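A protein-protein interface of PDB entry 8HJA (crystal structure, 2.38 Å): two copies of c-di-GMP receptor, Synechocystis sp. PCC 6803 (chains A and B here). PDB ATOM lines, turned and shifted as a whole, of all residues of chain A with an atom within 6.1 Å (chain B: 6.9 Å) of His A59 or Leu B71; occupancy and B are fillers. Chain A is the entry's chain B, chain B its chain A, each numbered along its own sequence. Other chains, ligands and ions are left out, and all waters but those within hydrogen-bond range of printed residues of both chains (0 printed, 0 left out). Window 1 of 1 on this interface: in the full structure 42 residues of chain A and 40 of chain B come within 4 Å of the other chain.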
ATOM      1  N   PRO A  18     -34.221 -17.959  22.936  1.00  0.00           N
ATOM      2  CA  PRO A  18     -34.345 -17.953  24.403  1.00  0.00           C
ATOM      3  C   PRO A  18     -35.683 -17.748  25.122  1.00  0.00           C
ATOM      4  O   PRO A  18     -35.866 -18.281  26.219  1.00  0.00           O
ATOM      5  CB  PRO A  18     -33.518 -16.711  24.782  1.00  0.00           C
ATOM      6  CG  PRO A  18     -32.395 -16.720  23.782  1.00  0.00           C
ATOM      7  CD  PRO A  18     -33.054 -17.173  22.493  1.00  0.00           C
ATOM      8  N   GLU A  21     -37.272 -20.981  24.022  1.00  0.00           N
ATOM      9  CA  GLU A  21     -36.351 -22.122  24.268  1.00  0.00           C
ATOM     10  C   GLU A  21     -36.600 -22.504  25.730  1.00  0.00           C
ATOM     11  O   GLU A  21     -36.788 -23.708  25.998  1.00  0.00           O
ATOM     12  CB  GLU A  21     -34.903 -21.722  23.974  1.00  0.00           C
ATOM     13  CG  GLU A  21     -33.931 -22.064  25.087  1.00  0.00           C
ATOM     14  CD  GLU A  21     -33.268 -20.853  25.717  1.00  0.00           C
ATOM     15  OE1 GLU A  21     -32.237 -20.400  25.182  1.00  0.00           O
ATOM     16  OE2 GLU A  21     -33.789 -20.363  26.738  1.00  0.00           O
ATOM     17  N   MET A  57     -30.085 -23.198  20.326  1.00  0.00           N
ATOM     18  CA  MET A  57     -29.120 -22.379  21.069  1.00  0.00           C
ATOM     19  C   MET A  57     -27.988 -23.109  21.784  1.00  0.00           C
ATOM     20  O   MET A  57     -28.247 -24.013  22.578  1.00  0.00           O
ATOM     21  CB  MET A  57     -29.755 -21.733  22.312  1.00  0.00           C
ATOM     22  CG  MET A  57     -30.880 -20.750  22.054  1.00  0.00           C
ATOM     23  SD  MET A  57     -30.352 -19.312  20.785  1.00  0.00           S
ATOM     24  CE  MET A  57     -30.606 -20.292  19.082  1.00  0.00           C
ATOM     25  N   PRO A  58     -26.709 -22.723  21.543  1.00  0.00           N
ATOM     26  CA  PRO A  58     -25.550 -23.407  22.157  1.00  0.00           C
ATOM     27  C   PRO A  58     -25.159 -22.715  23.479  1.00  0.00           C
ATOM     28  O   PRO A  58     -24.502 -21.674  23.470  1.00  0.00           O
ATOM     29  CB  PRO A  58     -24.531 -23.141  21.031  1.00  0.00           C
ATOM     30  CG  PRO A  58     -24.813 -21.701  20.632  1.00  0.00           C
ATOM     31  CD  PRO A  58     -26.319 -21.555  20.738  1.00  0.00           C
ATOM     32  N   HIS A  59     -25.549 -23.272  24.621  1.00  0.00           N
ATOM     33  CA  HIS A  59     -25.171 -22.653  25.922  1.00  0.00           C
ATOM     34  C   HIS A  59     -24.014 -23.429  26.524  1.00  0.00           C
ATOM     35  O   HIS A  59     -23.283 -22.933  27.396  1.00  0.00           O
ATOM     36  CB  HIS A  59     -26.328 -22.728  26.907  1.00  0.00           C
ATOM     37  CG  HIS A  59     -27.556 -22.027  26.456  1.00  0.00           C
ATOM     38  ND1 HIS A  59     -28.218 -21.114  27.245  1.00  0.00           N
ATOM     39  CD2 HIS A  59     -28.238 -22.104  25.314  1.00  0.00           C
ATOM     40  CE1 HIS A  59     -29.268 -20.661  26.586  1.00  0.00           C
ATOM     41  NE2 HIS A  59     -29.289 -21.242  25.410  1.00  0.00           N
ATOM     42  N   LYS A  60     -23.868 -24.648  26.051  1.00  0.00           N
ATOM     43  CA  LYS A  60     -22.822 -25.537  26.540  1.00  0.00           C
ATOM     44  C   LYS A  60     -21.444 -25.077  26.044  1.00  0.00           C
ATOM     45  O   LYS A  60     -20.430 -25.249  26.734  1.00  0.00           O
ATOM     46  CB  LYS A  60     -23.095 -26.974  26.069  1.00  0.00           C
ATOM     47  CG  LYS A  60     -24.254 -27.705  26.743  1.00  0.00           C
ATOM     48  CD  LYS A  60     -25.631 -27.359  26.192  1.00  0.00           C
ATOM     49  CE  LYS A  60     -25.802 -27.688  24.720  1.00  0.00           C
ATOM     50  NZ  LYS A  60     -26.569 -26.641  24.000  1.00  0.00           N
ATOM     51  N   LYS A  61     -21.434 -24.488  24.840  1.00  0.00           N
ATOM     52  CA  LYS A  61     -20.221 -24.281  24.080  1.00  0.00           C
ATOM     53  C   LYS A  61     -19.512 -22.996  24.526  1.00  0.00           C
ATOM     54  O   LYS A  61     -18.427 -22.721  24.039  1.00  0.00           O
ATOM     55  CB  LYS A  61     -20.546 -24.288  22.583  1.00  0.00           C
ATOM     56  CG  LYS A  61     -20.645 -25.658  21.911  1.00  0.00           C
ATOM     57  CD  LYS A  61     -21.920 -26.420  22.250  1.00  0.00           C
ATOM     58  CE  LYS A  61     -22.099 -27.735  21.513  1.00  0.00           C
ATOM     59  NZ  LYS A  61     -23.542 -28.075  21.328  1.00  0.00           N
ATOM     60  N   PHE A  62     -20.084 -22.203  25.439  1.00  0.00           N
ATOM     61  CA  PHE A  62     -19.413 -20.992  25.886  1.00  0.00           C
ATOM     62  C   PHE A  62     -19.537 -20.891  27.401  1.00  0.00           C
ATOM     63  O   PHE A  62     -20.535 -21.355  27.949  1.00  0.00           O
ATOM     64  CB  PHE A  62     -19.898 -19.724  25.162  1.00  0.00           C
ATOM     65  CG  PHE A  62     -21.262 -19.190  25.510  1.00  0.00           C
ATOM     66  CD1 PHE A  62     -21.479 -18.479  26.667  1.00  0.00           C
ATOM     67  CD2 PHE A  62     -22.356 -19.443  24.692  1.00  0.00           C
ATOM     68  CE1 PHE A  62     -22.743 -18.002  26.975  1.00  0.00           C
ATOM     69  CE2 PHE A  62     -23.616 -18.953  25.000  1.00  0.00           C
ATOM     70  CZ  PHE A  62     -23.794 -18.204  26.125  1.00  0.00           C
ATOM     71  N   ILE A  63     -18.494 -20.365  28.063  1.00  0.00           N
ATOM     72  CA  ILE A  63     -18.575 -20.110  29.493  1.00  0.00           C
ATOM     73  C   ILE A  63     -17.718 -18.911  29.887  1.00  0.00           C
ATOM     74  O   ILE A  63     -16.665 -18.668  29.311  1.00  0.00           O
ATOM     75  CB  ILE A  63     -18.160 -21.360  30.289  1.00  0.00           C
ATOM     76  CG1 ILE A  63     -18.664 -21.270  31.738  1.00  0.00           C
ATOM     77  CG2 ILE A  63     -16.655 -21.610  30.183  1.00  0.00           C
ATOM     78  CD1 ILE A  63     -18.497 -22.563  32.551  1.00  0.00           C
ATOM     79  N   ILE B  63     -27.029 -16.522  37.331  1.00  0.00           N
ATOM     80  CA  ILE B  63     -26.975 -16.519  35.883  1.00  0.00           C
ATOM     81  C   ILE B  63     -26.681 -15.101  35.423  1.00  0.00           C
ATOM     82  O   ILE B  63     -27.049 -14.148  36.103  1.00  0.00           O
ATOM     83  CB  ILE B  63     -28.257 -17.113  35.260  1.00  0.00           C
ATOM     84  CG1 ILE B  63     -27.963 -17.462  33.790  1.00  0.00           C
ATOM     85  CG2 ILE B  63     -29.463 -16.190  35.460  1.00  0.00           C
ATOM     86  CD1 ILE B  63     -29.121 -17.997  32.944  1.00  0.00           C
ATOM     87  N   MET B  66     -27.377 -11.266  30.850  1.00  0.00           N
ATOM     88  CA  MET B  66     -26.955 -10.687  29.585  1.00  0.00           C
ATOM     89  C   MET B  66     -26.830 -11.749  28.480  1.00  0.00           C
ATOM     90  O   MET B  66     -26.821 -11.405  27.291  1.00  0.00           O
ATOM     91  CB  MET B  66     -25.646  -9.902  29.776  1.00  0.00           C
ATOM     92  CG  MET B  66     -25.075  -9.246  28.494  1.00  0.00           C
ATOM     93  SD  MET B  66     -26.366  -7.954  27.714  1.00  0.00           S
ATOM     94  CE  MET B  66     -25.761  -6.302  28.597  1.00  0.00           C
ATOM     95  N   GLU B  67     -26.634 -13.022  28.854  1.00  0.00           N
ATOM     96  CA  GLU B  67     -26.565 -14.118  27.889  1.00  0.00           C
ATOM     97  C   GLU B  67     -27.917 -14.292  27.187  1.00  0.00           C
ATOM     98  O   GLU B  67     -27.962 -14.543  26.002  1.00  0.00           O
ATOM     99  CB  GLU B  67     -26.141 -15.427  28.557  1.00  0.00           C
ATOM    100  CG  GLU B  67     -24.715 -15.444  29.090  1.00  0.00           C
ATOM    101  CD  GLU B  67     -24.400 -16.572  30.078  1.00  0.00           C
ATOM    102  OE1 GLU B  67     -25.186 -17.523  30.136  1.00  0.00           O
ATOM    103  OE2 GLU B  67     -23.405 -16.469  30.852  1.00  0.00           O
ATOM    104  N   GLU B  68     -29.029 -14.161  27.905  1.00  0.00           N
ATOM    105  CA  GLU B  68     -30.349 -14.221  27.292  1.00  0.00           C
ATOM    106  C   GLU B  68     -30.512 -13.130  26.220  1.00  0.00           C
ATOM    107  O   GLU B  68     -30.893 -13.402  25.088  1.00  0.00           O
ATOM    108  CB  GLU B  68     -31.371 -14.074  28.415  1.00  0.00           C
ATOM    109  CG  GLU B  68     -32.825 -14.246  28.043  1.00  0.00           C
ATOM    110  CD  GLU B  68     -33.733 -13.853  29.203  1.00  0.00           C
ATOM    111  OE1 GLU B  68     -33.406 -14.259  30.369  1.00  0.00           O
ATOM    112  OE2 GLU B  68     -34.731 -13.083  28.961  1.00  0.00           O
ATOM    113  N   MET B  69     -30.230 -11.879  26.600  1.00  0.00           N
ATOM    114  CA  MET B  69     -30.292 -10.723  25.722  1.00  0.00           C
ATOM    115  C   MET B  69     -29.386 -10.921  24.516  1.00  0.00           C
ATOM    116  O   MET B  69     -29.737 -10.636  23.387  1.00  0.00           O
ATOM    117  CB  MET B  69     -29.821  -9.453  26.430  1.00  0.00           C
ATOM    118  CG  MET B  69     -30.260  -9.284  27.874  1.00  0.00           C
ATOM    119  SD  MET B  69     -32.226  -9.219  27.994  1.00  0.00           S
ATOM    120  CE  MET B  69     -32.484  -7.443  27.213  1.00  0.00           C
ATOM    121  N   VAL B  70     -28.211 -11.459  24.728  1.00  0.00           N
ATOM    122  CA  VAL B  70     -27.284 -11.514  23.629  1.00  0.00           C
ATOM    123  C   VAL B  70     -27.744 -12.584  22.639  1.00  0.00           C
ATOM    124  O   VAL B  70     -27.722 -12.360  21.429  1.00  0.00           O
ATOM    125  CB  VAL B  70     -25.841 -11.680  24.140  1.00  0.00           C
ATOM    126  CG1 VAL B  70     -24.901 -12.255  23.095  1.00  0.00           C
ATOM    127  CG2 VAL B  70     -25.329 -10.339  24.637  1.00  0.00           C
ATOM    128  N   LEU B  71     -28.169 -13.731  23.165  1.00  0.00           N
ATOM    129  CA  LEU B  71     -28.564 -14.884  22.358  1.00  0.00           C
ATOM    130  C   LEU B  71     -29.770 -14.520  21.478  1.00  0.00           C
ATOM    131  O   LEU B  71     -29.804 -14.880  20.300  1.00  0.00           O
ATOM    132  CB  LEU B  71     -28.857 -16.078  23.280  1.00  0.00           C
ATOM    133  CG  LEU B  71     -27.618 -16.804  23.810  1.00  0.00           C
ATOM    134  CD1 LEU B  71     -28.025 -17.827  24.861  1.00  0.00           C
ATOM    135  CD2 LEU B  71     -26.826 -17.480  22.670  1.00  0.00           C
ATOM    136  N   THR B  72     -30.697 -13.763  22.069  1.00  0.00           N
ATOM    137  CA  THR B  72     -31.883 -13.305  21.387  1.00  0.00           C
ATOM    138  C   THR B  72     -31.508 -12.306  20.295  1.00  0.00           C
ATOM    139  O   THR B  72     -32.157 -12.299  19.265  1.00  0.00           O
ATOM    140  CB  THR B  72     -32.847 -12.692  22.394  1.00  0.00           C
ATOM    141  OG1 THR B  72     -33.168 -13.727  23.312  1.00  0.00           O
ATOM    142  CG2 THR B  72     -34.103 -12.114  21.782  1.00  0.00           C
ATOM    143  N   GLU B  73     -30.462 -11.487  20.501  1.00  0.00           N
ATOM    144  CA  GLU B  73     -30.069 -10.499  19.507  1.00  0.00           C
ATOM    145  C   GLU B  73     -29.316 -11.185  18.383  1.00  0.00           C
ATOM    146  O   GLU B  73     -29.431 -10.752  17.258  1.00  0.00           O
ATOM    147  CB  GLU B  73     -29.272  -9.344  20.133  1.00  0.00           C
ATOM    148  CG  GLU B  73     -28.792  -8.276  19.159  1.00  0.00           C
ATOM    149  CD  GLU B  73     -29.843  -7.433  18.432  1.00  0.00           C
ATOM    150  OE1 GLU B  73     -30.996  -7.257  18.956  1.00  0.00           O
ATOM    151  OE2 GLU B  73     -29.519  -6.962  17.308  1.00  0.00           O
ATOM    152  N   VAL B  74     -28.588 -12.260  18.671  1.00  0.00           N
ATOM    153  CA  VAL B  74     -27.783 -12.935  17.658  1.00  0.00           C
ATOM    154  C   VAL B  74     -28.694 -13.658  16.653  1.00  0.00           C
ATOM    155  O   VAL B  74     -28.448 -13.625  15.439  1.00  0.00           O
ATOM    156  CB  VAL B  74     -26.794 -13.935  18.275  1.00  0.00           C
ATOM    157  CG1 VAL B  74     -25.983 -14.592  17.179  1.00  0.00           C
ATOM    158  CG2 VAL B  74     -25.889 -13.331  19.364  1.00  0.00           C
ATOM    159  N   VAL B  75     -29.707 -14.353  17.191  1.00  0.00           N
ATOM    160  CA  VAL B  75     -30.723 -15.025  16.397  1.00  0.00           C
ATOM    161  C   VAL B  75     -31.393 -13.983  15.500  1.00  0.00           C
ATOM    162  O   VAL B  75     -31.524 -14.176  14.308  1.00  0.00           O
ATOM    163  CB  VAL B  75     -31.768 -15.768  17.275  1.00  0.00           C
ATOM    164  CG1 VAL B  75     -32.959 -16.261  16.442  1.00  0.00           C
ATOM    165  CG2 VAL B  75     -31.127 -16.918  18.011  1.00  0.00           C
ATOM    166  N   SER B  76     -31.808 -12.874  16.086  1.00  0.00           N
ATOM    167  CA  SER B  76     -32.371 -11.770  15.334  1.00  0.00           C
ATOM    168  C   SER B  76     -31.480 -11.324  14.172  1.00  0.00           C
ATOM    169  O   SER B  76     -32.009 -10.996  13.109  1.00  0.00           O
ATOM    170  CB  SER B  76     -32.644 -10.631  16.259  1.00  0.00           C
ATOM    171  OG  SER B  76     -33.154  -9.543  15.525  1.00  0.00           O
ATOM    172  N   ILE B  91     -23.313 -19.438  16.653  1.00  0.00           N
ATOM    173  CA  ILE B  91     -23.986 -18.591  17.615  1.00  0.00           C
ATOM    174  C   ILE B  91     -23.104 -18.370  18.841  1.00  0.00           C
ATOM    175  O   ILE B  91     -23.067 -17.253  19.360  1.00  0.00           O
ATOM    176  CB  ILE B  91     -25.370 -19.181  17.946  1.00  0.00           C
ATOM    177  CG1 ILE B  91     -26.284 -19.033  16.718  1.00  0.00           C
ATOM    178  CG2 ILE B  91     -25.972 -18.557  19.192  1.00  0.00           C
ATOM    179  CD1 ILE B  91     -27.732 -19.519  16.880  1.00  0.00           C
ATOM    180  N   ALA B  92     -22.432 -19.429  19.309  1.00  0.00           N
ATOM    181  CA  ALA B  92     -21.638 -19.397  20.526  1.00  0.00           C
ATOM    182  C   ALA B  92     -20.515 -18.394  20.343  1.00  0.00           C
ATOM    183  O   ALA B  92     -20.325 -17.566  21.222  1.00  0.00           O
ATOM    184  CB  ALA B  92     -21.078 -20.773  20.854  1.00  0.00           C
ATOM    185  N   ALA B  95     -21.859 -14.774  20.361  1.00  0.00           N
ATOM    186  CA  ALA B  95     -22.373 -14.282  21.647  1.00  0.00           C
ATOM    187  C   ALA B  95     -21.214 -14.092  22.642  1.00  0.00           C
ATOM    188  O   ALA B  95     -21.156 -13.105  23.381  1.00  0.00           O
ATOM    189  CB  ALA B  95     -23.422 -15.233  22.222  1.00  0.00           C
ATOM    190  N   LEU B  99     -20.333 -10.795  24.612  1.00  0.00           N
ATOM    191  CA  LEU B  99     -20.492 -10.884  26.057  1.00  0.00           C
ATOM    192  C   LEU B  99     -19.252 -10.335  26.738  1.00  0.00           C
ATOM    193  O   LEU B  99     -19.328  -9.674  27.770  1.00  0.00           O
ATOM    194  CB  LEU B  99     -20.773 -12.336  26.460  1.00  0.00           C
ATOM    195  CG  LEU B  99     -22.246 -12.763  26.355  1.00  0.00           C
ATOM    196  CD1 LEU B  99     -22.399 -14.281  26.315  1.00  0.00           C
ATOM    197  CD2 LEU B  99     -23.045 -12.207  27.529  1.00  0.00           C
ATOM    198  N   ILE B 128     -25.774  -3.457  22.857  1.00  0.00           N
ATOM    199  CA  ILE B 128     -25.870  -4.885  22.595  1.00  0.00           C
ATOM    200  C   ILE B 128     -25.894  -5.167  21.104  1.00  0.00           C
ATOM    201  O   ILE B 128     -25.151  -6.039  20.647  1.00  0.00           O
ATOM    202  CB  ILE B 128     -27.084  -5.493  23.312  1.00  0.00           C
ATOM    203  CG1 ILE B 128     -26.915  -5.383  24.823  1.00  0.00           C
ATOM    204  CG2 ILE B 128     -27.310  -6.943  22.883  1.00  0.00           C
ATOM    205  CD1 ILE B 128     -28.198  -5.573  25.574  1.00  0.00           C
ATOM    206  N   VAL B 132     -23.167  -7.317  19.033  1.00  0.00           N
ATOM    207  CA  VAL B 132     -23.519  -8.543  18.329  1.00  0.00           C
ATOM    208  C   VAL B 132     -23.139  -8.415  16.854  1.00  0.00           C
ATOM    209  O   VAL B 132     -22.554  -9.348  16.303  1.00  0.00           O
ATOM    210  CB  VAL B 132     -24.981  -8.927  18.573  1.00  0.00           C
ATOM    211  CG1 VAL B 132     -25.460 -10.003  17.594  1.00  0.00           C
ATOM    212  CG2 VAL B 132     -25.200  -9.372  20.018  1.00  0.00           C
ATOM    213  N   GLU B 152     -17.655 -28.348  25.974  1.00  0.00           N
ATOM    214  CA  GLU B 152     -18.975 -29.029  25.909  1.00  0.00           C
ATOM    215  C   GLU B 152     -19.558 -29.142  27.318  1.00  0.00           C
ATOM    216  O   GLU B 152     -20.793 -29.232  27.401  1.00  0.00           O
ATOM    217  CB  GLU B 152     -18.835 -30.410  25.273  1.00  0.00           C
ATOM    218  CG  GLU B 152     -19.026 -30.412  23.772  1.00  0.00           C
ATOM    219  CD  GLU B 152     -17.850 -30.997  23.011  1.00  0.00           C
ATOM    220  OE1 GLU B 152     -17.719 -32.234  22.991  1.00  0.00           O
ATOM    221  OE2 GLU B 152     -17.064 -30.215  22.454  1.00  0.00           O
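Among the printed residues, merely in contact across the chains: Pro A18 with Thr B72 (3.1 Å), Pro A58 with Ile B91 (3.4 Å), Lys A60 with Glu B152 (3.5 Å), His A59 with Leu B71 (3.5 Å), Pro A58 with Ala B92 (3.5 Å), Met A57 with Val B75 (3.6 Å), Pro A18 with Leu B71 (3.6 Å), Met A57 with Ile B91 (3.7 Å), Phe A62 with Leu B99 (3.8 Å), Phe A62 with Glu B67 (3.8 Å), Pro A18 with Glu B68 (3.9 Å) and Lys A61 with Ala B92 (3.95 Å).
Position printed for both chains: 63. Of the 12 pairs that touch across the chains among the printed residues, none has its exchanged pair printed and touching as well.
Of the 19 printed residues of chain B, 9 touch a printed residue of chain A. Hydrophobic or aromatic side chains of chain B within 4 Å of the printed part of chain A: Leu B71, Val B75, Ile B91, Ala B92 and Leu B99. Along chain A the printed residues that touch a printed residue of chain B span positions 18 to 62. Among the printed residues, 12 pairs touch across the chains.
The side-chain carboxylate (OE1) of Glu A21 lies within hydrogen-bond range of a ring nitrogen (NE2) of His A59 (3.1 Å). The backbone carbonyl oxygen of Glu B68 is in hydrogen-bond range of the side-chain hydroxyl of Thr B72, 2.9 Å away. The side-chain amino group (NZ) of Lys A60 is in hydrogen-bond range of the backbone carbonyl oxygen (O) of Met A57 (3.4 Å).
Of the printed residues of chain B, Met A57 touches Val B75 (3.6 Å) and Ile B91 (3.7 Å). Of the printed residues of chain B, Phe A62 touches Glu B67 and Leu B99. Of the printed residues of chain A, Glu B67 touches Phe A62. Met B69 touches none of the printed residues of chain A. Of the printed residues of chain A, Val B75 touches Met A57 (3.6 Å). Of the printed residues of chain A, Ile B91 touches Met A57 (3.7 Å) and Pro A58 (3.4 Å). The nearest printed residue of chain A that does not touch Glu B152 is Lys A61 (4.7 Å).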
